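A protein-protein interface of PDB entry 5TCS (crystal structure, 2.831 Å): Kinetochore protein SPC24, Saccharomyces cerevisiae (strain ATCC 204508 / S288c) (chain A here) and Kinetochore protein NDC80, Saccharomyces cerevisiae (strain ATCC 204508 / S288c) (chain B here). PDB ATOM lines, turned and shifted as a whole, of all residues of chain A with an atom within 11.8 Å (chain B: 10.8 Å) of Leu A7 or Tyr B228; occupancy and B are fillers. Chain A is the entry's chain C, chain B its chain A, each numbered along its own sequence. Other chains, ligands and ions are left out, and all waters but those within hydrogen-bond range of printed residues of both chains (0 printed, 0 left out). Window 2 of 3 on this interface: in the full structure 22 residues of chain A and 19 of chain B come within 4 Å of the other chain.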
ATOM      1  N   LYS A   4     -28.526 -38.274  24.714  1.00  0.00           N
ATOM      2  CA  LYS A   4     -27.449 -38.680  23.820  1.00  0.00           C
ATOM      3  C   LYS A   4     -26.093 -38.277  24.393  1.00  0.00           C
ATOM      4  O   LYS A   4     -25.913 -37.148  24.849  1.00  0.00           O
ATOM      5  CB  LYS A   4     -27.649 -38.065  22.433  1.00  0.00           C
ATOM      6  CG  LYS A   4     -28.879 -38.589  21.705  1.00  0.00           C
ATOM      7  CD  LYS A   4     -29.054 -37.930  20.346  1.00  0.00           C
ATOM      8  CE  LYS A   4     -30.257 -38.495  19.609  1.00  0.00           C
ATOM      9  NZ  LYS A   4     -30.469 -37.833  18.293  1.00  0.00           N
ATOM     10  N   ASP A   5     -25.141 -39.208  24.368  1.00  0.00           N
ATOM     11  CA  ASP A   5     -23.824 -38.975  24.941  1.00  0.00           C
ATOM     12  C   ASP A   5     -22.930 -38.255  23.936  1.00  0.00           C
ATOM     13  O   ASP A   5     -23.307 -38.009  22.786  1.00  0.00           O
ATOM     14  CB  ASP A   5     -23.208 -40.296  25.397  1.00  0.00           C
ATOM     15  CG  ASP A   5     -24.003 -40.956  26.505  1.00  0.00           C
ATOM     16  OD1 ASP A   5     -24.623 -40.226  27.308  1.00  0.00           O
ATOM     17  OD2 ASP A   5     -24.009 -42.203  26.576  1.00  0.00           O
ATOM     18  N   ASN A   6     -21.716 -37.908  24.373  1.00  0.00           N
ATOM     19  CA  ASN A   6     -20.858 -36.974  23.647  1.00  0.00           C
ATOM     20  C   ASN A   6     -21.594 -35.665  23.368  1.00  0.00           C
ATOM     21  O   ASN A   6     -21.252 -34.930  22.434  1.00  0.00           O
ATOM     22  CB  ASN A   6     -20.332 -37.591  22.344  1.00  0.00           C
ATOM     23  CG  ASN A   6     -19.007 -38.304  22.536  1.00  0.00           C
ATOM     24  OD1 ASN A   6     -18.106 -37.793  23.204  1.00  0.00           O
ATOM     25  ND2 ASN A   6     -18.880 -39.491  21.955  1.00  0.00           N
ATOM     26  N   LEU A   7     -22.600 -35.377  24.190  1.00  0.00           N
ATOM     27  CA  LEU A   7     -23.468 -34.214  24.027  1.00  0.00           C
ATOM     28  C   LEU A   7     -23.765 -33.699  25.427  1.00  0.00           C
ATOM     29  O   LEU A   7     -24.421 -34.391  26.214  1.00  0.00           O
ATOM     30  CB  LEU A   7     -24.753 -34.592  23.291  1.00  0.00           C
ATOM     31  CG  LEU A   7     -25.526 -33.476  22.589  1.00  0.00           C
ATOM     32  CD1 LEU A   7     -24.792 -33.020  21.337  1.00  0.00           C
ATOM     33  CD2 LEU A   7     -26.934 -33.944  22.254  1.00  0.00           C
ATOM     34  N   LEU A   8     -23.275 -32.504  25.745  1.00  0.00           N
ATOM     35  CA  LEU A   8     -23.386 -31.976  27.100  1.00  0.00           C
ATOM     36  C   LEU A   8     -24.832 -32.007  27.572  1.00  0.00           C
ATOM     37  O   LEU A   8     -25.740 -31.549  26.872  1.00  0.00           O
ATOM     38  CB  LEU A   8     -22.840 -30.549  27.152  1.00  0.00           C
ATOM     39  CG  LEU A   8     -21.360 -30.407  26.795  1.00  0.00           C
ATOM     40  CD1 LEU A   8     -20.990 -28.938  26.670  1.00  0.00           C
ATOM     41  CD2 LEU A   8     -20.485 -31.100  27.831  1.00  0.00           C
ATOM     42  N   ASP A   9     -25.039 -32.556  28.772  1.00  0.00           N
ATOM     43  CA  ASP A   9     -26.391 -32.696  29.299  1.00  0.00           C
ATOM     44  C   ASP A   9     -27.016 -31.336  29.584  1.00  0.00           C
ATOM     45  O   ASP A   9     -28.218 -31.141  29.372  1.00  0.00           O
ATOM     46  CB  ASP A   9     -26.370 -33.566  30.555  1.00  0.00           C
ATOM     47  CG  ASP A   9     -25.572 -34.841  30.361  1.00  0.00           C
ATOM     48  OD1 ASP A   9     -26.119 -35.807  29.788  1.00  0.00           O
ATOM     49  OD2 ASP A   9     -24.395 -34.876  30.778  1.00  0.00           O
ATOM     50  N   ASN A  10     -26.221 -30.379  30.065  1.00  0.00           N
ATOM     51  CA  ASN A  10     -26.657 -28.986  30.164  1.00  0.00           C
ATOM     52  C   ASN A  10     -25.426 -28.104  30.003  1.00  0.00           C
ATOM     53  O   ASN A  10     -24.661 -27.909  30.961  1.00  0.00           O
ATOM     54  CB  ASN A  10     -27.373 -28.691  31.479  1.00  0.00           C
ATOM     55  CG  ASN A  10     -27.977 -27.298  31.508  1.00  0.00           C
ATOM     56  OD1 ASN A  10     -27.871 -26.543  30.539  1.00  0.00           O
ATOM     57  ND2 ASN A  10     -28.627 -26.955  32.612  1.00  0.00           N
ATOM     58  N   PRO A  11     -25.209 -27.536  28.813  1.00  0.00           N
ATOM     59  CA  PRO A  11     -23.965 -26.772  28.601  1.00  0.00           C
ATOM     60  C   PRO A  11     -23.951 -25.430  29.304  1.00  0.00           C
ATOM     61  O   PRO A  11     -22.905 -25.029  29.836  1.00  0.00           O
ATOM     62  CB  PRO A  11     -23.918 -26.621  27.074  1.00  0.00           C
ATOM     63  CG  PRO A  11     -25.357 -26.626  26.664  1.00  0.00           C
ATOM     64  CD  PRO A  11     -26.061 -27.556  27.611  1.00  0.00           C
ATOM     65  N   VAL A  12     -25.076 -24.712  29.317  1.00  0.00           N
ATOM     66  CA  VAL A  12     -25.149 -23.437  30.029  1.00  0.00           C
ATOM     67  C   VAL A  12     -24.640 -23.604  31.454  1.00  0.00           C
ATOM     68  O   VAL A  12     -23.754 -22.869  31.916  1.00  0.00           O
ATOM     69  CB  VAL A  12     -26.596 -22.903  30.001  1.00  0.00           C
ATOM     70  CG1 VAL A  12     -26.723 -21.602  30.775  1.00  0.00           C
ATOM     71  CG2 VAL A  12     -27.052 -22.691  28.564  1.00  0.00           C
ATOM     72  N   GLU A  13     -25.195 -24.580  32.172  1.00  0.00           N
ATOM     73  CA  GLU A  13     -24.793 -24.819  33.552  1.00  0.00           C
ATOM     74  C   GLU A  13     -23.315 -25.173  33.655  1.00  0.00           C
ATOM     75  O   GLU A  13     -22.678 -24.875  34.673  1.00  0.00           O
ATOM     76  CB  GLU A  13     -25.660 -25.928  34.149  1.00  0.00           C
ATOM     77  CG  GLU A  13     -25.344 -26.264  35.597  1.00  0.00           C
ATOM     78  CD  GLU A  13     -24.523 -27.531  35.744  1.00  0.00           C
ATOM     79  OE1 GLU A  13     -24.700 -28.459  34.926  1.00  0.00           O
ATOM     80  OE2 GLU A  13     -23.701 -27.600  36.681  1.00  0.00           O
ATOM     81  N   PHE A  14     -22.749 -25.805  32.624  1.00  0.00           N
ATOM     82  CA  PHE A  14     -21.323 -26.116  32.650  1.00  0.00           C
ATOM     83  C   PHE A  14     -20.485 -24.849  32.538  1.00  0.00           C
ATOM     84  O   PHE A  14     -19.574 -24.623  33.343  1.00  0.00           O
ATOM     85  CB  PHE A  14     -20.968 -27.097  31.529  1.00  0.00           C
ATOM     86  CG  PHE A  14     -21.313 -28.529  31.835  1.00  0.00           C
ATOM     87  CD1 PHE A  14     -20.798 -29.157  32.957  1.00  0.00           C
ATOM     88  CD2 PHE A  14     -22.133 -29.255  30.987  1.00  0.00           C
ATOM     89  CE1 PHE A  14     -21.109 -30.474  33.239  1.00  0.00           C
ATOM     90  CE2 PHE A  14     -22.449 -30.573  31.262  1.00  0.00           C
ATOM     91  CZ  PHE A  14     -21.935 -31.183  32.389  1.00  0.00           C
ATOM     92  N   LEU B 219     -34.390 -30.376   8.234  1.00  0.00           N
ATOM     93  CA  LEU B 219     -34.054 -29.435   9.296  1.00  0.00           C
ATOM     94  C   LEU B 219     -33.558 -30.174  10.529  1.00  0.00           C
ATOM     95  O   LEU B 219     -32.468 -29.889  11.042  1.00  0.00           O
ATOM     96  CB  LEU B 219     -35.266 -28.570   9.640  1.00  0.00           C
ATOM     97  CG  LEU B 219     -35.055 -27.590  10.799  1.00  0.00           C
ATOM     98  CD1 LEU B 219     -33.864 -26.681  10.532  1.00  0.00           C
ATOM     99  CD2 LEU B 219     -36.307 -26.766  11.045  1.00  0.00           C
ATOM    100  N   LYS B 220     -34.348 -31.135  11.012  1.00  0.00           N
ATOM    101  CA  LYS B 220     -33.916 -31.996  12.104  1.00  0.00           C
ATOM    102  C   LYS B 220     -32.443 -32.350  11.948  1.00  0.00           C
ATOM    103  O   LYS B 220     -31.601 -31.942  12.758  1.00  0.00           O
ATOM    104  CB  LYS B 220     -34.776 -33.266  12.143  1.00  0.00           C
ATOM    105  CG  LYS B 220     -36.249 -33.031  12.445  1.00  0.00           C
ATOM    106  CD  LYS B 220     -37.009 -34.351  12.490  1.00  0.00           C
ATOM    107  CE  LYS B 220     -38.387 -34.196  13.115  1.00  0.00           C
ATOM    108  NZ  LYS B 220     -39.483 -34.581  12.182  1.00  0.00           N
ATOM    109  N   VAL B 221     -32.119 -33.076  10.873  1.00  0.00           N
ATOM    110  CA  VAL B 221     -30.736 -33.478  10.621  1.00  0.00           C
ATOM    111  C   VAL B 221     -29.808 -32.289  10.819  1.00  0.00           C
ATOM    112  O   VAL B 221     -28.903 -32.310  11.663  1.00  0.00           O
ATOM    113  CB  VAL B 221     -30.595 -34.067   9.206  1.00  0.00           C
ATOM    114  CG1 VAL B 221     -29.137 -34.410   8.905  1.00  0.00           C
ATOM    115  CG2 VAL B 221     -31.477 -35.300   9.045  1.00  0.00           C
ATOM    116  N   ASP B 222     -30.050 -31.219  10.057  1.00  0.00           N
ATOM    117  CA  ASP B 222     -29.209 -30.031  10.144  1.00  0.00           C
ATOM    118  C   ASP B 222     -28.996 -29.625  11.594  1.00  0.00           C
ATOM    119  O   ASP B 222     -27.856 -29.494  12.056  1.00  0.00           O
ATOM    120  CB  ASP B 222     -29.841 -28.887   9.352  1.00  0.00           C
ATOM    121  CG  ASP B 222     -28.848 -27.795   9.016  1.00  0.00           C
ATOM    122  OD1 ASP B 222     -27.737 -28.126   8.553  1.00  0.00           O
ATOM    123  OD2 ASP B 222     -29.179 -26.607   9.217  1.00  0.00           O
ATOM    124  N   LEU B 223     -30.087 -29.456  12.343  1.00  0.00           N
ATOM    125  CA  LEU B 223     -29.957 -29.008  13.724  1.00  0.00           C
ATOM    126  C   LEU B 223     -29.099 -29.978  14.526  1.00  0.00           C
ATOM    127  O   LEU B 223     -28.179 -29.565  15.242  1.00  0.00           O
ATOM    128  CB  LEU B 223     -31.340 -28.847  14.358  1.00  0.00           C
ATOM    129  CG  LEU B 223     -32.245 -27.778  13.733  1.00  0.00           C
ATOM    130  CD1 LEU B 223     -33.557 -27.680  14.496  1.00  0.00           C
ATOM    131  CD2 LEU B 223     -31.561 -26.417  13.684  1.00  0.00           C
ATOM    132  N   ASN B 224     -29.367 -31.281  14.395  1.00  0.00           N
ATOM    133  CA  ASN B 224     -28.574 -32.263  15.124  1.00  0.00           C
ATOM    134  C   ASN B 224     -27.093 -32.120  14.806  1.00  0.00           C
ATOM    135  O   ASN B 224     -26.247 -32.333  15.682  1.00  0.00           O
ATOM    136  CB  ASN B 224     -29.056 -33.677  14.800  1.00  0.00           C
ATOM    137  CG  ASN B 224     -30.441 -33.959  15.350  1.00  0.00           C
ATOM    138  OD1 ASN B 224     -30.952 -33.217  16.186  1.00  0.00           O
ATOM    139  ND2 ASN B 224     -31.051 -35.045  14.887  1.00  0.00           N
ATOM    140  N   ARG B 225     -26.760 -31.749  13.569  1.00  0.00           N
ATOM    141  CA  ARG B 225     -25.359 -31.551  13.217  1.00  0.00           C
ATOM    142  C   ARG B 225     -24.807 -30.291  13.869  1.00  0.00           C
ATOM    143  O   ARG B 225     -23.671 -30.286  14.358  1.00  0.00           O
ATOM    144  CB  ARG B 225     -25.202 -31.487  11.698  1.00  0.00           C
ATOM    145  CG  ARG B 225     -25.453 -32.815  11.007  1.00  0.00           C
ATOM    146  CD  ARG B 225     -25.212 -32.735   9.509  1.00  0.00           C
ATOM    147  NE  ARG B 225     -25.423 -34.032   8.878  1.00  0.00           N
ATOM    148  CZ  ARG B 225     -25.348 -34.261   7.570  1.00  0.00           C
ATOM    149  NH1 ARG B 225     -25.063 -33.279   6.726  1.00  0.00           N
ATOM    150  NH2 ARG B 225     -25.558 -35.484   7.108  1.00  0.00           N
ATOM    151  N   LYS B 226     -25.598 -29.217  13.900  1.00  0.00           N
ATOM    152  CA  LYS B 226     -25.120 -27.971  14.487  1.00  0.00           C
ATOM    153  C   LYS B 226     -24.959 -28.108  15.997  1.00  0.00           C
ATOM    154  O   LYS B 226     -23.913 -27.756  16.555  1.00  0.00           O
ATOM    155  CB  LYS B 226     -26.076 -26.827  14.147  1.00  0.00           C
ATOM    156  CG  LYS B 226     -26.291 -26.607  12.653  1.00  0.00           C
ATOM    157  CD  LYS B 226     -26.334 -25.118  12.304  1.00  0.00           C
ATOM    158  CE  LYS B 226     -27.495 -24.755  11.384  1.00  0.00           C
ATOM    159  NZ  LYS B 226     -27.114 -24.757   9.944  1.00  0.00           N
ATOM    160  N   ARG B 227     -25.991 -28.620  16.671  1.00  0.00           N
ATOM    161  CA  ARG B 227     -25.935 -28.828  18.114  1.00  0.00           C
ATOM    162  C   ARG B 227     -24.628 -29.494  18.522  1.00  0.00           C
ATOM    163  O   ARG B 227     -23.863 -28.953  19.330  1.00  0.00           O
ATOM    164  CB  ARG B 227     -27.133 -29.668  18.553  1.00  0.00           C
ATOM    165  CG  ARG B 227     -27.172 -29.989  20.040  1.00  0.00           C
ATOM    166  CD  ARG B 227     -28.554 -29.726  20.601  1.00  0.00           C
ATOM    167  NE  ARG B 227     -29.593 -30.345  19.777  1.00  0.00           N
ATOM    168  CZ  ARG B 227     -30.764 -29.789  19.476  1.00  0.00           C
ATOM    169  NH1 ARG B 227     -31.073 -28.575  19.917  1.00  0.00           N
ATOM    170  NH2 ARG B 227     -31.631 -30.447  18.719  1.00  0.00           N
ATOM    171  N   TYR B 228     -24.357 -30.680  17.973  1.00  0.00           N
ATOM    172  CA  TYR B 228     -23.077 -31.333  18.213  1.00  0.00           C
ATOM    173  C   TYR B 228     -21.932 -30.356  17.980  1.00  0.00           C
ATOM    174  O   TYR B 228     -21.150 -30.060  18.891  1.00  0.00           O
ATOM    175  CB  TYR B 228     -22.939 -32.561  17.308  1.00  0.00           C
ATOM    176  CG  TYR B 228     -21.613 -33.273  17.450  1.00  0.00           C
ATOM    177  CD1 TYR B 228     -21.413 -34.215  18.453  1.00  0.00           C
ATOM    178  CD2 TYR B 228     -20.560 -33.003  16.587  1.00  0.00           C
ATOM    179  CE1 TYR B 228     -20.202 -34.866  18.591  1.00  0.00           C
ATOM    180  CE2 TYR B 228     -19.345 -33.650  16.716  1.00  0.00           C
ATOM    181  CZ  TYR B 228     -19.171 -34.581  17.721  1.00  0.00           C
ATOM    182  OH  TYR B 228     -17.965 -35.230  17.856  1.00  0.00           O
ATOM    183  N   LYS B 229     -21.846 -29.819  16.759  1.00  0.00           N
ATOM    184  CA  LYS B 229     -20.805 -28.850  16.431  1.00  0.00           C
ATOM    185  C   LYS B 229     -20.673 -27.797  17.523  1.00  0.00           C
ATOM    186  O   LYS B 229     -19.559 -27.408  17.893  1.00  0.00           O
ATOM    187  CB  LYS B 229     -21.123 -28.182  15.093  1.00  0.00           C
ATOM    188  CG  LYS B 229     -19.909 -27.848  14.240  1.00  0.00           C
ATOM    189  CD  LYS B 229     -19.374 -29.082  13.525  1.00  0.00           C
ATOM    190  CE  LYS B 229     -18.472 -28.708  12.357  1.00  0.00           C
ATOM    191  NZ  LYS B 229     -19.224 -28.030  11.260  1.00  0.00           N
ATOM    192  N   LEU B 230     -21.803 -27.331  18.057  1.00  0.00           N
ATOM    193  CA  LEU B 230     -21.763 -26.306  19.091  1.00  0.00           C
ATOM    194  C   LEU B 230     -21.220 -26.866  20.396  1.00  0.00           C
ATOM    195  O   LEU B 230     -20.294 -26.300  20.987  1.00  0.00           O
ATOM    196  CB  LEU B 230     -23.159 -25.718  19.304  1.00  0.00           C
ATOM    197  CG  LEU B 230     -23.255 -24.614  20.359  1.00  0.00           C
ATOM    198  CD1 LEU B 230     -22.376 -23.428  19.987  1.00  0.00           C
ATOM    199  CD2 LEU B 230     -24.698 -24.176  20.541  1.00  0.00           C
ATOM    200  N   HIS B 231     -21.785 -27.978  20.867  1.00  0.00           N
ATOM    201  CA  HIS B 231     -21.361 -28.516  22.155  1.00  0.00           C
ATOM    202  C   HIS B 231     -19.857 -28.749  22.170  1.00  0.00           C
ATOM    203  O   HIS B 231     -19.166 -28.359  23.120  1.00  0.00           O
ATOM    204  CB  HIS B 231     -22.127 -29.802  22.465  1.00  0.00           C
ATOM    205  CG  HIS B 231     -23.535 -29.564  22.913  1.00  0.00           C
ATOM    206  ND1 HIS B 231     -24.275 -30.514  23.585  1.00  0.00           N
ATOM    207  CD2 HIS B 231     -24.339 -28.481  22.788  1.00  0.00           C
ATOM    208  CE1 HIS B 231     -25.474 -30.026  23.853  1.00  0.00           C
ATOM    209  NE2 HIS B 231     -25.539 -28.794  23.380  1.00  0.00           N
ATOM    210  N   GLN B 232     -19.327 -29.356  21.106  1.00  0.00           N
ATOM    211  CA  GLN B 232     -17.882 -29.501  20.973  1.00  0.00           C
ATOM    212  C   GLN B 232     -17.182 -28.186  21.297  1.00  0.00           C
ATOM    213  O   GLN B 232     -16.357 -28.116  22.217  1.00  0.00           O
ATOM    214  CB  GLN B 232     -17.532 -29.972  19.559  1.00  0.00           C
ATOM    215  CG  GLN B 232     -18.129 -31.323  19.184  1.00  0.00           C
ATOM    216  CD  GLN B 232     -17.660 -32.446  20.091  1.00  0.00           C
ATOM    217  OE1 GLN B 232     -18.459 -33.068  20.793  1.00  0.00           O
ATOM    218  NE2 GLN B 232     -16.362 -32.716  20.076  1.00  0.00           N
ATOM    219  N   GLN B 233     -17.524 -27.122  20.565  1.00  0.00           N
ATOM    220  CA  GLN B 233     -16.973 -25.801  20.844  1.00  0.00           C
ATOM    221  C   GLN B 233     -16.982 -25.512  22.340  1.00  0.00           C
ATOM    222  O   GLN B 233     -15.937 -25.231  22.938  1.00  0.00           O
ATOM    223  CB  GLN B 233     -17.756 -24.721  20.089  1.00  0.00           C
ATOM    224  CG  GLN B 233     -17.508 -24.682  18.593  1.00  0.00           C
ATOM    225  CD  GLN B 233     -18.266 -23.556  17.916  1.00  0.00           C
ATOM    226  OE1 GLN B 233     -19.495 -23.497  17.971  1.00  0.00           O
ATOM    227  NE2 GLN B 233     -17.533 -22.647  17.283  1.00  0.00           N
ATOM    228  N   VAL B 234     -18.161 -25.598  22.965  1.00  0.00           N
ATOM    229  CA  VAL B 234     -18.263 -25.358  24.403  1.00  0.00           C
ATOM    230  C   VAL B 234     -17.222 -26.195  25.136  1.00  0.00           C
ATOM    231  O   VAL B 234     -16.359 -25.672  25.847  1.00  0.00           O
ATOM    232  CB  VAL B 234     -19.687 -25.658  24.901  1.00  0.00           C
ATOM    233  CG1 VAL B 234     -19.705 -25.944  26.401  1.00  0.00           C
ATOM    234  CG2 VAL B 234     -20.597 -24.482  24.587  1.00  0.00           C
ATOM    235  N   ILE B 235     -17.271 -27.510  24.942  1.00  0.00           N
ATOM    236  CA  ILE B 235     -16.317 -28.438  25.541  1.00  0.00           C
ATOM    237  C   ILE B 235     -14.926 -27.840  25.360  1.00  0.00           C
ATOM    238  O   ILE B 235     -14.199 -27.627  26.341  1.00  0.00           O
ATOM    239  CB  ILE B 235     -16.420 -29.845  24.911  1.00  0.00           C
ATOM    240  CG1 ILE B 235     -17.638 -30.572  25.479  1.00  0.00           C
ATOM    241  CG2 ILE B 235     -15.154 -30.659  25.164  1.00  0.00           C
ATOM    242  CD1 ILE B 235     -18.258 -31.569  24.530  1.00  0.00           C
ATOM    243  N   HIS B 236     -14.573 -27.542  24.109  1.00  0.00           N
ATOM    244  CA  HIS B 236     -13.249 -27.011  23.818  1.00  0.00           C
ATOM    245  C   HIS B 236     -12.879 -25.908  24.802  1.00  0.00           C
ATOM    246  O   HIS B 236     -11.866 -26.004  25.505  1.00  0.00           O
ATOM    247  CB  HIS B 236     -13.184 -26.499  22.378  1.00  0.00           C
ATOM    248  CG  HIS B 236     -11.822 -26.039  21.954  1.00  0.00           C
ATOM    249  ND1 HIS B 236     -10.677 -26.762  22.212  1.00  0.00           N
ATOM    250  CD2 HIS B 236     -11.424 -24.926  21.293  1.00  0.00           C
ATOM    251  CE1 HIS B 236      -9.632 -26.115  21.726  1.00  0.00           C
ATOM    252  NE2 HIS B 236     -10.057 -24.998  21.164  1.00  0.00           N
ATOM    253  N   ILE B 238     -14.226 -25.006  27.702  1.00  0.00           N
ATOM    254  CA  ILE B 238     -14.191 -25.515  29.069  1.00  0.00           C
ATOM    255  C   ILE B 238     -12.925 -26.315  29.295  1.00  0.00           C
ATOM    256  O   ILE B 238     -12.408 -26.374  30.418  1.00  0.00           O
ATOM    257  CB  ILE B 238     -15.455 -26.349  29.371  1.00  0.00           C
ATOM    258  CG1 ILE B 238     -16.677 -25.426  29.452  1.00  0.00           C
ATOM    259  CG2 ILE B 238     -15.277 -27.157  30.665  1.00  0.00           C
ATOM    260  CD1 ILE B 238     -17.964 -26.104  29.907  1.00  0.00           C
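The backbone NH of Leu A8 is in hydrogen-bond range of a ring nitrogen (ND1) of His B231 (3.1 Å).
Among the printed residues, pairs that only touch across the chains: Leu A8 with Val B234 (3.3 Å), Leu A7 with His B231 (3.4 Å), Phe A14 with Ile B238 (3.6 Å), Leu A8 with Ile B235 (3.7 Å), Asn A6 with Gln B232 (3.7 Å), Pro A11 with His B231 (3.9 Å), Leu A7 with Tyr B228 (3.9 Å) and Asn A6 with Tyr B228 (3.98 Å).
Of chain B, only Tyr B228 (3.9 Å) and His B231 (3.4 Å) come within 4 Å of Leu A7. Of chain B, only His B231, Val B234 and Ile B235 come within 4 Å of Leu A8. No residue of chain B comes within 4 Å of Asp A9. Of the printed residues of chain B, Phe A14 touches Ile B238. No residue of chain A comes within 4 Å of Arg B227. Printed residues of chain A within 4 Å of Tyr B228: Asn A6 and Leu A7. No residue of chain A comes within 4 Å of Lys B229. Of chain A, only Asn A6 (3.7 Å) comes within 4 Å of Gln B232. Printed residues of chain A within 4 Å of Ile B235: Leu A8 (3.7 Å). The nearest residue of chain B that does not touch Leu A7 is Arg B227 (4.1 Å).
Printed residues of chain B that touch a printed residue of chain A: Tyr B228, His B231, Gln B232, Val B234, Ile B235 and Ile B238. Hydrophobic or aromatic side chains of chain B within 4 Å of the printed part of chain A: Tyr B228, His B231, Val B234, Ile B235 and Ile B238. Along chain B the printed residues that touch a printed residue of chain A span positions 228 to 238. Of the 11 printed residues of chain A, 5 touch a printed residue of chain B. Printed residues of chain A that touch a printed residue of chain B: Asn A6, Leu A7, Leu A8, Pro A11 and Phe A14. Among the printed residues, 9 pairs touch across the chains.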
